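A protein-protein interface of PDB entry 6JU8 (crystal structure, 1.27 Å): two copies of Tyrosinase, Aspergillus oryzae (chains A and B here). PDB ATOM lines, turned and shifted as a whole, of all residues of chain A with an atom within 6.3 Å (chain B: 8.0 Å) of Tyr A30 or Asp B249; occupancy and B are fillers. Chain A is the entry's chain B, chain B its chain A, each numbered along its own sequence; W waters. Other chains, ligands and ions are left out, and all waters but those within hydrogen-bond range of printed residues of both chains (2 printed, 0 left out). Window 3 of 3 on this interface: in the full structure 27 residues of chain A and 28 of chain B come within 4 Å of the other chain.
The side-chain carboxylate (OD2) of Asp B249 sits at hydrogen-bond distance from the side-chain hydroxyl (OH) of Tyr A30 (2.6 Å).
The side-chain hydroxyl (OH) of Tyr A30 sits close to the side-chain sulfur (SD) of Met A176, at 3.4 Å.
The side-chain amide oxygen (OD1) of Asn B247 is in hydrogen-bond range of the backbone NH (N) of Asp B249, 2.7 Å away.
The backbone carbonyl oxygen (O) of Tyr A30 is in hydrogen-bond range of the side-chain hydroxyl (OG1) of Thr A34 (3.0 Å).
Among the printed residues, pairs that only touch across the chains: Leu A31 with Asn B247, Met A176 with Asp B249 and Pro A177 with Asp B253.
Ile A26 touches none of the printed residues of chain B.
Of the printed residues of chain B, Leu A31 touches Asn B247.
Leu A43 touches none of the printed residues of chain B.
Printed residues of chain B within 4 Å of Met A176: Asp B249 (3.8 Å).
Of the printed residues of chain B, Pro A177 touches Asp B253.
Of chain A, only Tyr A30 (2.6 Å) and Met A176 (3.8 Å) come within 4 Å of Asp B249.
Printed residues of chain A within 4 Å of Asp B253: Pro A177 (3.5 Å).
The nearest printed residue of chain B that does not touch Met A176 is Val B250 (4.4 Å).
Printed residues of chain A that touch a printed residue of chain B: Tyr A30, Leu A31, Met A176 and Pro A177.
Hydrophobic or aromatic side chains of chain A that line the printed part of chain B: Tyr A30, Leu A31, Met A176 and Pro A177.
Among the printed residues, no Asp or Glu carboxylate lies within 4 Å of a Lys or Arg side-chain nitrogen of the other chain.
No position is printed for both chains.
Water W2 lies within hydrogen-bond range of the side-chain hydroxyl of Thr A34 (2.8 Å), the side-chain carboxylate of Asp B249 (2.9 Å) and the side-chain amide nitrogen of Asn B247 (3.2 Å).
Water W1 bridges OD2 of Asp B249 (2.9 Å) and NH2 of Arg A40 (3.0 Å).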
ATOM      1  N   ASP A  25      14.826  25.159  11.845  1.00  0.00           N
ATOM      2  CA  ASP A  25      14.527  24.980  10.428  1.00  0.00           C
ATOM      3  C   ASP A  25      13.230  25.731  10.129  1.00  0.00           C
ATOM      4  O   ASP A  25      12.214  25.519  10.798  1.00  0.00           O
ATOM      5  CB  ASP A  25      14.381  23.501  10.133  1.00  0.00           C
ATOM      6  CG  ASP A  25      13.994  23.110   8.728  1.00  0.00           C
ATOM      7  OD1 ASP A  25      12.999  23.650   8.198  1.00  0.00           O
ATOM      8  OD2 ASP A  25      14.615  22.192   8.153  1.00  0.00           O
ATOM      9  N   ILE A  26      13.256  26.620   9.137  1.00  0.00           N
ATOM     10  CA  ILE A  26      12.093  27.479   8.907  1.00  0.00           C
ATOM     11  C   ILE A  26      10.828  26.729   8.525  1.00  0.00           C
ATOM     12  O   ILE A  26       9.721  27.205   8.792  1.00  0.00           O
ATOM     13  CB  ILE A  26      12.414  28.561   7.846  1.00  0.00           C
ATOM     14  CG1 ILE A  26      11.347  29.663   7.868  1.00  0.00           C
ATOM     15  CG2 ILE A  26      12.663  27.969   6.468  1.00  0.00           C
ATOM     16  CD1 ILE A  26      11.709  30.989   7.290  1.00  0.00           C
ATOM     17  N   ASP A  27      10.935  25.574   7.868  1.00  0.00           N
ATOM     18  CA  ASP A  27       9.718  24.801   7.579  1.00  0.00           C
ATOM     19  C   ASP A  27       9.176  24.190   8.862  1.00  0.00           C
ATOM     20  O   ASP A  27       7.975  24.225   9.150  1.00  0.00           O
ATOM     21  CB  ASP A  27       9.995  23.738   6.503  1.00  0.00           C
ATOM     22  CG  ASP A  27       9.882  24.277   5.089  1.00  0.00           C
ATOM     23  OD1 ASP A  27       9.565  25.469   4.893  1.00  0.00           O
ATOM     24  OD2 ASP A  27      10.087  23.483   4.154  1.00  0.00           O
ATOM     25  N   ASP A  28      10.045  23.605   9.702  1.00  0.00           N
ATOM     26  CA  ASP A  28       9.567  23.043  10.968  1.00  0.00           C
ATOM     27  C   ASP A  28       8.930  24.135  11.829  1.00  0.00           C
ATOM     28  O   ASP A  28       7.873  23.938  12.435  1.00  0.00           O
ATOM     29  CB  ASP A  28      10.707  22.367  11.728  1.00  0.00           C
ATOM     30  CG  ASP A  28      11.193  21.079  11.095  1.00  0.00           C
ATOM     31  OD1 ASP A  28      10.512  20.525  10.211  1.00  0.00           O
ATOM     32  OD2 ASP A  28      12.283  20.623  11.500  1.00  0.00           O
ATOM     33  N   TRP A  29       9.583  25.294  11.863  1.00  0.00           N
ATOM     34  CA  TRP A  29       9.129  26.422  12.674  1.00  0.00           C
ATOM     35  C   TRP A  29       7.774  26.916  12.169  1.00  0.00           C
ATOM     36  O   TRP A  29       6.846  27.132  12.955  1.00  0.00           O
ATOM     37  CB  TRP A  29      10.191  27.523  12.655  1.00  0.00           C
ATOM     38  CG  TRP A  29       9.817  28.816  13.314  1.00  0.00           C
ATOM     39  CD1 TRP A  29       9.922  29.127  14.636  1.00  0.00           C
ATOM     40  CD2 TRP A  29       9.285  29.971  12.668  1.00  0.00           C
ATOM     41  NE1 TRP A  29       9.470  30.415  14.872  1.00  0.00           N
ATOM     42  CE2 TRP A  29       9.081  30.955  13.664  1.00  0.00           C
ATOM     43  CE3 TRP A  29       8.951  30.272  11.339  1.00  0.00           C
ATOM     44  CZ2 TRP A  29       8.568  32.224  13.375  1.00  0.00           C
ATOM     45  CZ3 TRP A  29       8.440  31.539  11.070  1.00  0.00           C
ATOM     46  CH2 TRP A  29       8.251  32.498  12.070  1.00  0.00           C
ATOM     47  N   TYR A  30       7.623  27.076  10.851  1.00  0.00           N
ATOM     48  CA  TYR A  30       6.368  27.576  10.306  1.00  0.00           C
ATOM     49  C   TYR A  30       5.244  26.587  10.566  1.00  0.00           C
ATOM     50  O   TYR A  30       4.123  26.902  10.966  1.00  0.00           O
ATOM     51  CB  TYR A  30       6.539  27.876   8.790  1.00  0.00           C
ATOM     52  CG  TYR A  30       5.192  28.279   8.212  1.00  0.00           C
ATOM     53  CD1 TYR A  30       4.712  29.559   8.440  1.00  0.00           C
ATOM     54  CD2 TYR A  30       4.383  27.393   7.501  1.00  0.00           C
ATOM     55  CE1 TYR A  30       3.495  29.992   7.958  1.00  0.00           C
ATOM     56  CE2 TYR A  30       3.152  27.813   7.028  1.00  0.00           C
ATOM     57  CZ  TYR A  30       2.715  29.104   7.248  1.00  0.00           C
ATOM     58  OH  TYR A  30       1.484  29.531   6.808  1.00  0.00           O
ATOM     59  N   LEU A  31       5.504  25.288  10.343  1.00  0.00           N
ATOM     60  CA  LEU A  31       4.494  24.242  10.560  1.00  0.00           C
ATOM     61  C   LEU A  31       4.072  24.156  12.029  1.00  0.00           C
ATOM     62  O   LEU A  31       2.906  23.930  12.362  1.00  0.00           O
ATOM     63  CB  LEU A  31       5.046  22.901  10.078  1.00  0.00           C
ATOM     64  CG  LEU A  31       5.215  22.781   8.560  1.00  0.00           C
ATOM     65  CD1 LEU A  31       5.948  21.487   8.214  1.00  0.00           C
ATOM     66  CD2 LEU A  31       3.855  22.857   7.883  1.00  0.00           C
ATOM     67  N   GLU A  32       5.020  24.365  12.948  1.00  0.00           N
ATOM     68  CA  GLU A  32       4.720  24.423  14.370  1.00  0.00           C
ATOM     69  C   GLU A  32       3.851  25.647  14.694  1.00  0.00           C
ATOM     70  O   GLU A  32       2.820  25.521  15.357  1.00  0.00           O
ATOM     71  CB  GLU A  32       5.975  24.425  15.230  1.00  0.00           C
ATOM     72  CG  GLU A  32       5.724  24.394  16.738  1.00  0.00           C
ATOM     73  CD  GLU A  32       4.861  23.232  17.190  1.00  0.00           C
ATOM     74  OE1 GLU A  32       4.978  22.138  16.590  1.00  0.00           O
ATOM     75  OE2 GLU A  32       4.091  23.403  18.160  1.00  0.00           O
ATOM     76  N   GLN A  33       4.256  26.819  14.208  1.00  0.00           N
ATOM     77  CA  GLN A  33       3.571  28.076  14.493  1.00  0.00           C
ATOM     78  C   GLN A  33       2.132  28.100  14.012  1.00  0.00           C
ATOM     79  O   GLN A  33       1.280  28.752  14.634  1.00  0.00           O
ATOM     80  CB  GLN A  33       4.345  29.265  13.889  1.00  0.00           C
ATOM     81  CG  GLN A  33       5.606  29.584  14.684  1.00  0.00           C
ATOM     82  CD  GLN A  33       5.263  30.158  16.046  1.00  0.00           C
ATOM     83  OE1 GLN A  33       4.560  31.174  16.129  1.00  0.00           O
ATOM     84  NE2 GLN A  33       5.755  29.513  17.098  1.00  0.00           N
ATOM     85  N   THR A  34       1.874  27.366  12.938  1.00  0.00           N
ATOM     86  CA  THR A  34       0.551  27.324  12.324  1.00  0.00           C
ATOM     87  C   THR A  34      -0.245  26.100  12.764  1.00  0.00           C
ATOM     88  O   THR A  34      -1.354  25.906  12.259  1.00  0.00           O
ATOM     89  CB  THR A  34       0.598  27.393  10.790  1.00  0.00           C
ATOM     90  OG1 THR A  34       1.326  26.291  10.252  1.00  0.00           O
ATOM     91  CG2 THR A  34       1.298  28.679  10.363  1.00  0.00           C
ATOM     92  N   SER A  35       0.279  25.317  13.697  1.00  0.00           N
ATOM     93  CA  SER A  35      -0.465  24.197  14.252  1.00  0.00           C
ATOM     94  C   SER A  35      -1.315  24.643  15.433  1.00  0.00           C
ATOM     95  O   SER A  35      -1.058  25.667  16.091  1.00  0.00           O
ATOM     96  CB  SER A  35       0.501  23.078  14.662  1.00  0.00           C
ATOM     97  OG  SER A  35       1.100  23.444  15.918  1.00  0.00           O
ATOM     98  N   ARG A  40       1.158  30.812  18.016  1.00  0.00           N
ATOM     99  CA  ARG A  40       1.376  31.579  16.784  1.00  0.00           C
ATOM    100  C   ARG A  40       2.103  32.896  17.029  1.00  0.00           C
ATOM    101  O   ARG A  40       2.168  33.779  16.167  1.00  0.00           O
ATOM    102  CB  ARG A  40       0.051  31.845  16.042  1.00  0.00           C
ATOM    103  CG  ARG A  40       0.204  31.939  14.522  1.00  0.00           C
ATOM    104  CD  ARG A  40      -1.118  32.281  13.848  1.00  0.00           C
ATOM    105  NE  ARG A  40      -1.039  32.264  12.395  1.00  0.00           N
ATOM    106  CZ  ARG A  40      -1.375  31.252  11.603  1.00  0.00           C
ATOM    107  NH1 ARG A  40      -1.821  30.112  12.140  1.00  0.00           N
ATOM    108  NH2 ARG A  40      -1.251  31.375  10.286  1.00  0.00           N
ATOM    109  N   LEU A  43       5.536  33.570  14.932  1.00  0.00           N
ATOM    110  CA  LEU A  43       5.259  33.923  13.540  1.00  0.00           C
ATOM    111  C   LEU A  43       4.713  35.336  13.405  1.00  0.00           C
ATOM    112  O   LEU A  43       5.169  36.114  12.559  1.00  0.00           O
ATOM    113  CB  LEU A  43       4.272  32.921  12.935  1.00  0.00           C
ATOM    114  CG  LEU A  43       3.766  33.250  11.542  1.00  0.00           C
ATOM    115  CD1 LEU A  43       4.928  33.324  10.564  1.00  0.00           C
ATOM    116  CD2 LEU A  43       2.743  32.196  11.133  1.00  0.00           C
ATOM    117  N   ILE A 172       8.309  26.821   2.752  1.00  0.00           N
ATOM    118  CA  ILE A 172       6.874  27.065   2.608  1.00  0.00           C
ATOM    119  C   ILE A 172       6.539  28.540   2.673  1.00  0.00           C
ATOM    120  O   ILE A 172       5.874  29.130   1.803  1.00  0.00           O
ATOM    121  CB  ILE A 172       6.101  26.306   3.722  1.00  0.00           C
ATOM    122  CG1 ILE A 172       6.387  24.786   3.646  1.00  0.00           C
ATOM    123  CG2 ILE A 172       4.626  26.636   3.681  1.00  0.00           C
ATOM    124  CD1 ILE A 172       6.070  24.039   4.913  1.00  0.00           C
ATOM    125  N   LEU A 173       6.996  29.185   3.740  1.00  0.00           N
ATOM    126  CA  LEU A 173       6.593  30.553   4.030  1.00  0.00           C
ATOM    127  C   LEU A 173       7.119  31.485   2.945  1.00  0.00           C
ATOM    128  O   LEU A 173       6.462  32.458   2.628  1.00  0.00           O
ATOM    129  CB  LEU A 173       7.095  30.938   5.421  1.00  0.00           C
ATOM    130  CG  LEU A 173       6.727  32.344   5.909  1.00  0.00           C
ATOM    131  CD1 LEU A 173       5.246  32.617   5.756  1.00  0.00           C
ATOM    132  CD2 LEU A 173       7.184  32.468   7.356  1.00  0.00           C
ATOM    133  N   MET A 176       4.644  31.971  -0.053  1.00  0.00           N
ATOM    134  CA  MET A 176       3.289  32.452   0.212  1.00  0.00           C
ATOM    135  C   MET A 176       3.211  33.967   0.049  1.00  0.00           C
ATOM    136  O   MET A 176       3.915  34.692   0.773  1.00  0.00           O
ATOM    137  CB  MET A 176       2.900  32.102   1.663  1.00  0.00           C
ATOM    138  CG  MET A 176       2.729  30.597   1.886  1.00  0.00           C
ATOM    139  SD  MET A 176       2.604  30.151   3.629  1.00  0.00           S
ATOM    140  CE  MET A 176       1.285  31.236   4.139  1.00  0.00           C
ATOM    141  N   PRO A 177       2.390  34.489  -0.851  1.00  0.00           N
ATOM    142  CA  PRO A 177       2.278  35.952  -0.978  1.00  0.00           C
ATOM    143  C   PRO A 177       1.734  36.629   0.270  1.00  0.00           C
ATOM    144  O   PRO A 177       2.107  37.760   0.601  1.00  0.00           O
ATOM    145  CB  PRO A 177       1.326  36.145  -2.158  1.00  0.00           C
ATOM    146  CG  PRO A 177       1.278  34.848  -2.875  1.00  0.00           C
ATOM    147  CD  PRO A 177       1.623  33.768  -1.898  1.00  0.00           C
ATOM    148  N   MET A 178       0.819  35.961   0.958  1.00  0.00           N
ATOM    149  CA  MET A 178       0.152  36.471   2.151  1.00  0.00           C
ATOM    150  C   MET A 178       0.365  35.515   3.308  1.00  0.00           C
ATOM    151  O   MET A 178       0.586  34.317   3.123  1.00  0.00           O
ATOM    152  CB  MET A 178      -1.346  36.648   1.883  1.00  0.00           C
ATOM    153  CG  MET A 178      -1.733  37.537   0.715  1.00  0.00           C
ATOM    154  SD  MET A 178      -1.292  39.277   0.919  1.00  0.00           S
ATOM    155  CE  MET A 178      -2.563  39.900   2.000  1.00  0.00           C
ATOM    156  N   VAL A 179       0.284  36.019   4.533  1.00  0.00           N
ATOM    157  CA  VAL A 179       0.466  35.163   5.715  1.00  0.00           C
ATOM    158  C   VAL A 179      -0.481  35.663   6.803  1.00  0.00           C
ATOM    159  O   VAL A 179      -0.738  36.875   6.921  1.00  0.00           O
ATOM    160  CB  VAL A 179       1.925  35.218   6.191  1.00  0.00           C
ATOM    161  CG1 VAL A 179       2.338  36.640   6.589  1.00  0.00           C
ATOM    162  CG2 VAL A 179       2.157  34.258   7.348  1.00  0.00           C
ATOM    163  N   LYS A 180      -1.028  34.742   7.589  1.00  0.00           N
ATOM    164  CA  LYS A 180      -1.984  35.106   8.630  1.00  0.00           C
ATOM    165  C   LYS A 180      -1.273  35.211   9.972  1.00  0.00           C
ATOM    166  O   LYS A 180      -0.473  34.372  10.366  1.00  0.00           O
ATOM    167  CB  LYS A 180      -3.121  34.076   8.720  1.00  0.00           C
ATOM    168  CG  LYS A 180      -4.157  34.306   7.626  1.00  0.00           C
ATOM    169  CD  LYS A 180      -5.367  33.393   7.769  1.00  0.00           C
ATOM    170  CE  LYS A 180      -6.378  33.785   6.698  1.00  0.00           C
ATOM    171  NZ  LYS A 180      -5.983  33.306   5.343  1.00  0.00           N
ATOM    172  N   LEU B 205     -11.212  31.655   1.320  1.00  0.00           N
ATOM    173  CA  LEU B 205     -11.021  30.481   0.474  1.00  0.00           C
ATOM    174  C   LEU B 205     -12.314  30.185  -0.268  1.00  0.00           C
ATOM    175  O   LEU B 205     -13.399  30.272   0.306  1.00  0.00           O
ATOM    176  CB  LEU B 205     -10.598  29.270   1.302  1.00  0.00           C
ATOM    177  CG  LEU B 205      -9.324  29.410   2.146  1.00  0.00           C
ATOM    178  CD1 LEU B 205      -9.021  28.068   2.806  1.00  0.00           C
ATOM    179  CD2 LEU B 205      -8.148  29.923   1.353  1.00  0.00           C
ATOM    180  N   LYS B 233      -9.542  25.047  -1.656  1.00  0.00           N
ATOM    181  CA  LYS B 233      -8.511  25.565  -0.756  1.00  0.00           C
ATOM    182  C   LYS B 233      -7.808  26.791  -1.317  1.00  0.00           C
ATOM    183  O   LYS B 233      -6.870  27.314  -0.714  1.00  0.00           O
ATOM    184  CB  LYS B 233      -7.471  24.488  -0.444  1.00  0.00           C
ATOM    185  CG  LYS B 233      -8.036  23.225   0.161  1.00  0.00           C
ATOM    186  CD  LYS B 233      -8.774  23.475   1.460  1.00  0.00           C
ATOM    187  CE  LYS B 233      -9.261  22.176   2.094  1.00  0.00           C
ATOM    188  NZ  LYS B 233      -9.920  22.489   3.399  1.00  0.00           N
ATOM    189  N   TYR B 246       1.909  19.430  -1.128  1.00  0.00           N
ATOM    190  CA  TYR B 246       2.304  20.749  -0.659  1.00  0.00           C
ATOM    191  C   TYR B 246       1.327  21.231   0.404  1.00  0.00           C
ATOM    192  O   TYR B 246       0.143  20.945   0.393  1.00  0.00           O
ATOM    193  CB  TYR B 246       2.409  21.749  -1.811  1.00  0.00           C
ATOM    194  CG  TYR B 246       3.741  21.637  -2.516  1.00  0.00           C
ATOM    195  CD1 TYR B 246       4.150  20.464  -3.153  1.00  0.00           C
ATOM    196  CD2 TYR B 246       4.609  22.721  -2.531  1.00  0.00           C
ATOM    197  CE1 TYR B 246       5.388  20.385  -3.783  1.00  0.00           C
ATOM    198  CE2 TYR B 246       5.837  22.647  -3.150  1.00  0.00           C
ATOM    199  CZ  TYR B 246       6.225  21.480  -3.775  1.00  0.00           C
ATOM    200  OH  TYR B 246       7.457  21.457  -4.395  1.00  0.00           O
ATOM    201  N   ASN B 247       1.867  22.004   1.346  1.00  0.00           N
ATOM    202  CA  ASN B 247       1.042  22.589   2.403  1.00  0.00           C
ATOM    203  C   ASN B 247      -0.097  23.422   1.822  1.00  0.00           C
ATOM    204  O   ASN B 247       0.123  24.196   0.881  1.00  0.00           O
ATOM    205  CB  ASN B 247       1.924  23.439   3.317  1.00  0.00           C
ATOM    206  CG  ASN B 247       1.203  23.944   4.552  1.00  0.00           C
ATOM    207  OD1 ASN B 247       0.399  24.861   4.483  1.00  0.00           O
ATOM    208  ND2 ASN B 247       1.469  23.296   5.686  1.00  0.00           N
ATOM    209  N   ALA B 248      -1.288  23.298   2.387  1.00  0.00           N
ATOM    210  CA  ALA B 248      -2.480  23.967   1.858  1.00  0.00           C
ATOM    211  C   ALA B 248      -2.358  25.479   1.989  1.00  0.00           C
ATOM    212  O   ALA B 248      -3.051  26.231   1.276  1.00  0.00           O
ATOM    213  CB  ALA B 248      -3.722  23.490   2.598  1.00  0.00           C
ATOM    214  N   ASP B 249      -1.470  25.997   2.830  1.00  0.00           N
ATOM    215  CA  ASP B 249      -1.299  27.461   2.868  1.00  0.00           C
ATOM    216  C   ASP B 249      -0.656  27.957   1.579  1.00  0.00           C
ATOM    217  O   ASP B 249      -0.823  29.134   1.215  1.00  0.00           O
ATOM    218  CB  ASP B 249      -0.440  27.878   4.061  1.00  0.00           C
ATOM    219  CG  ASP B 249      -1.173  27.733   5.383  1.00  0.00           C
ATOM    220  OD1 ASP B 249      -2.402  27.488   5.407  1.00  0.00           O
ATOM    221  OD2 ASP B 249      -0.471  27.860   6.410  1.00  0.00           O
ATOM    222  N   VAL B 250       0.088  27.108   0.870  1.00  0.00           N
ATOM    223  CA  VAL B 250       0.600  27.466  -0.450  1.00  0.00           C
ATOM    224  C   VAL B 250      -0.556  27.524  -1.463  1.00  0.00           C
ATOM    225  O   VAL B 250      -0.667  28.453  -2.263  1.00  0.00           O
ATOM    226  CB  VAL B 250       1.681  26.466  -0.921  1.00  0.00           C
ATOM    227  CG1 VAL B 250       2.153  26.788  -2.332  1.00  0.00           C
ATOM    228  CG2 VAL B 250       2.861  26.529   0.043  1.00  0.00           C
ATOM    229  N   TRP B 251      -1.458  26.531  -1.404  1.00  0.00           N
ATOM    230  CA  TRP B 251      -2.606  26.443  -2.305  1.00  0.00           C
ATOM    231  C   TRP B 251      -3.513  27.661  -2.218  1.00  0.00           C
ATOM    232  O   TRP B 251      -4.227  27.978  -3.182  1.00  0.00           O
ATOM    233  CB  TRP B 251      -3.412  25.192  -1.947  1.00  0.00           C
ATOM    234  CG  TRP B 251      -2.688  23.907  -2.237  1.00  0.00           C
ATOM    235  CD1 TRP B 251      -1.530  23.678  -2.919  1.00  0.00           C
ATOM    236  CD2 TRP B 251      -3.155  22.630  -1.794  1.00  0.00           C
ATOM    237  NE1 TRP B 251      -1.276  22.323  -2.935  1.00  0.00           N
ATOM    238  CE2 TRP B 251      -2.243  21.649  -2.252  1.00  0.00           C
ATOM    239  CE3 TRP B 251      -4.276  22.239  -1.060  1.00  0.00           C
ATOM    240  CZ2 TRP B 251      -2.404  20.288  -2.001  1.00  0.00           C
ATOM    241  CZ3 TRP B 251      -4.438  20.886  -0.807  1.00  0.00           C
ATOM    242  CH2 TRP B 251      -3.511  19.920  -1.273  1.00  0.00           C
ATOM    243  N   ALA B 252      -3.547  28.364  -1.089  1.00  0.00           N
ATOM    244  CA  ALA B 252      -4.421  29.529  -0.967  1.00  0.00           C
ATOM    245  C   ALA B 252      -4.131  30.527  -2.080  1.00  0.00           C
ATOM    246  O   ALA B 252      -5.033  31.171  -2.628  1.00  0.00           O
ATOM    247  CB  ALA B 252      -4.174  30.181   0.387  1.00  0.00           C
ATOM    248  N   ASP B 253      -2.844  30.676  -2.408  1.00  0.00           N
ATOM    249  CA  ASP B 253      -2.460  31.508  -3.558  1.00  0.00           C
ATOM    250  C   ASP B 253      -1.149  30.927  -4.091  1.00  0.00           C
ATOM    251  O   ASP B 253      -0.075  31.211  -3.561  1.00  0.00           O
ATOM    252  CB  ASP B 253      -2.289  32.968  -3.170  1.00  0.00           C
ATOM    253  CG  ASP B 253      -1.990  33.876  -4.352  1.00  0.00           C
ATOM    254  OD1 ASP B 253      -1.655  33.365  -5.436  1.00  0.00           O
ATOM    255  OD2 ASP B 253      -2.072  35.111  -4.189  1.00  0.00           O
ATOM    256  N   GLY B 254      -1.262  30.081  -5.099  1.00  0.00           N
ATOM    257  CA  GLY B 254      -0.149  29.361  -5.655  1.00  0.00           C
ATOM    258  C   GLY B 254       0.668  30.127  -6.662  1.00  0.00           C
ATOM    259  O   GLY B 254       1.677  29.623  -7.167  1.00  0.00           O
HETATM  260  O   HOH W   1      -1.870  28.936   8.667  1.00  0.00           O
HETATM  261  O   HOH W   2       0.347  25.435   7.776  1.00  0.00           O
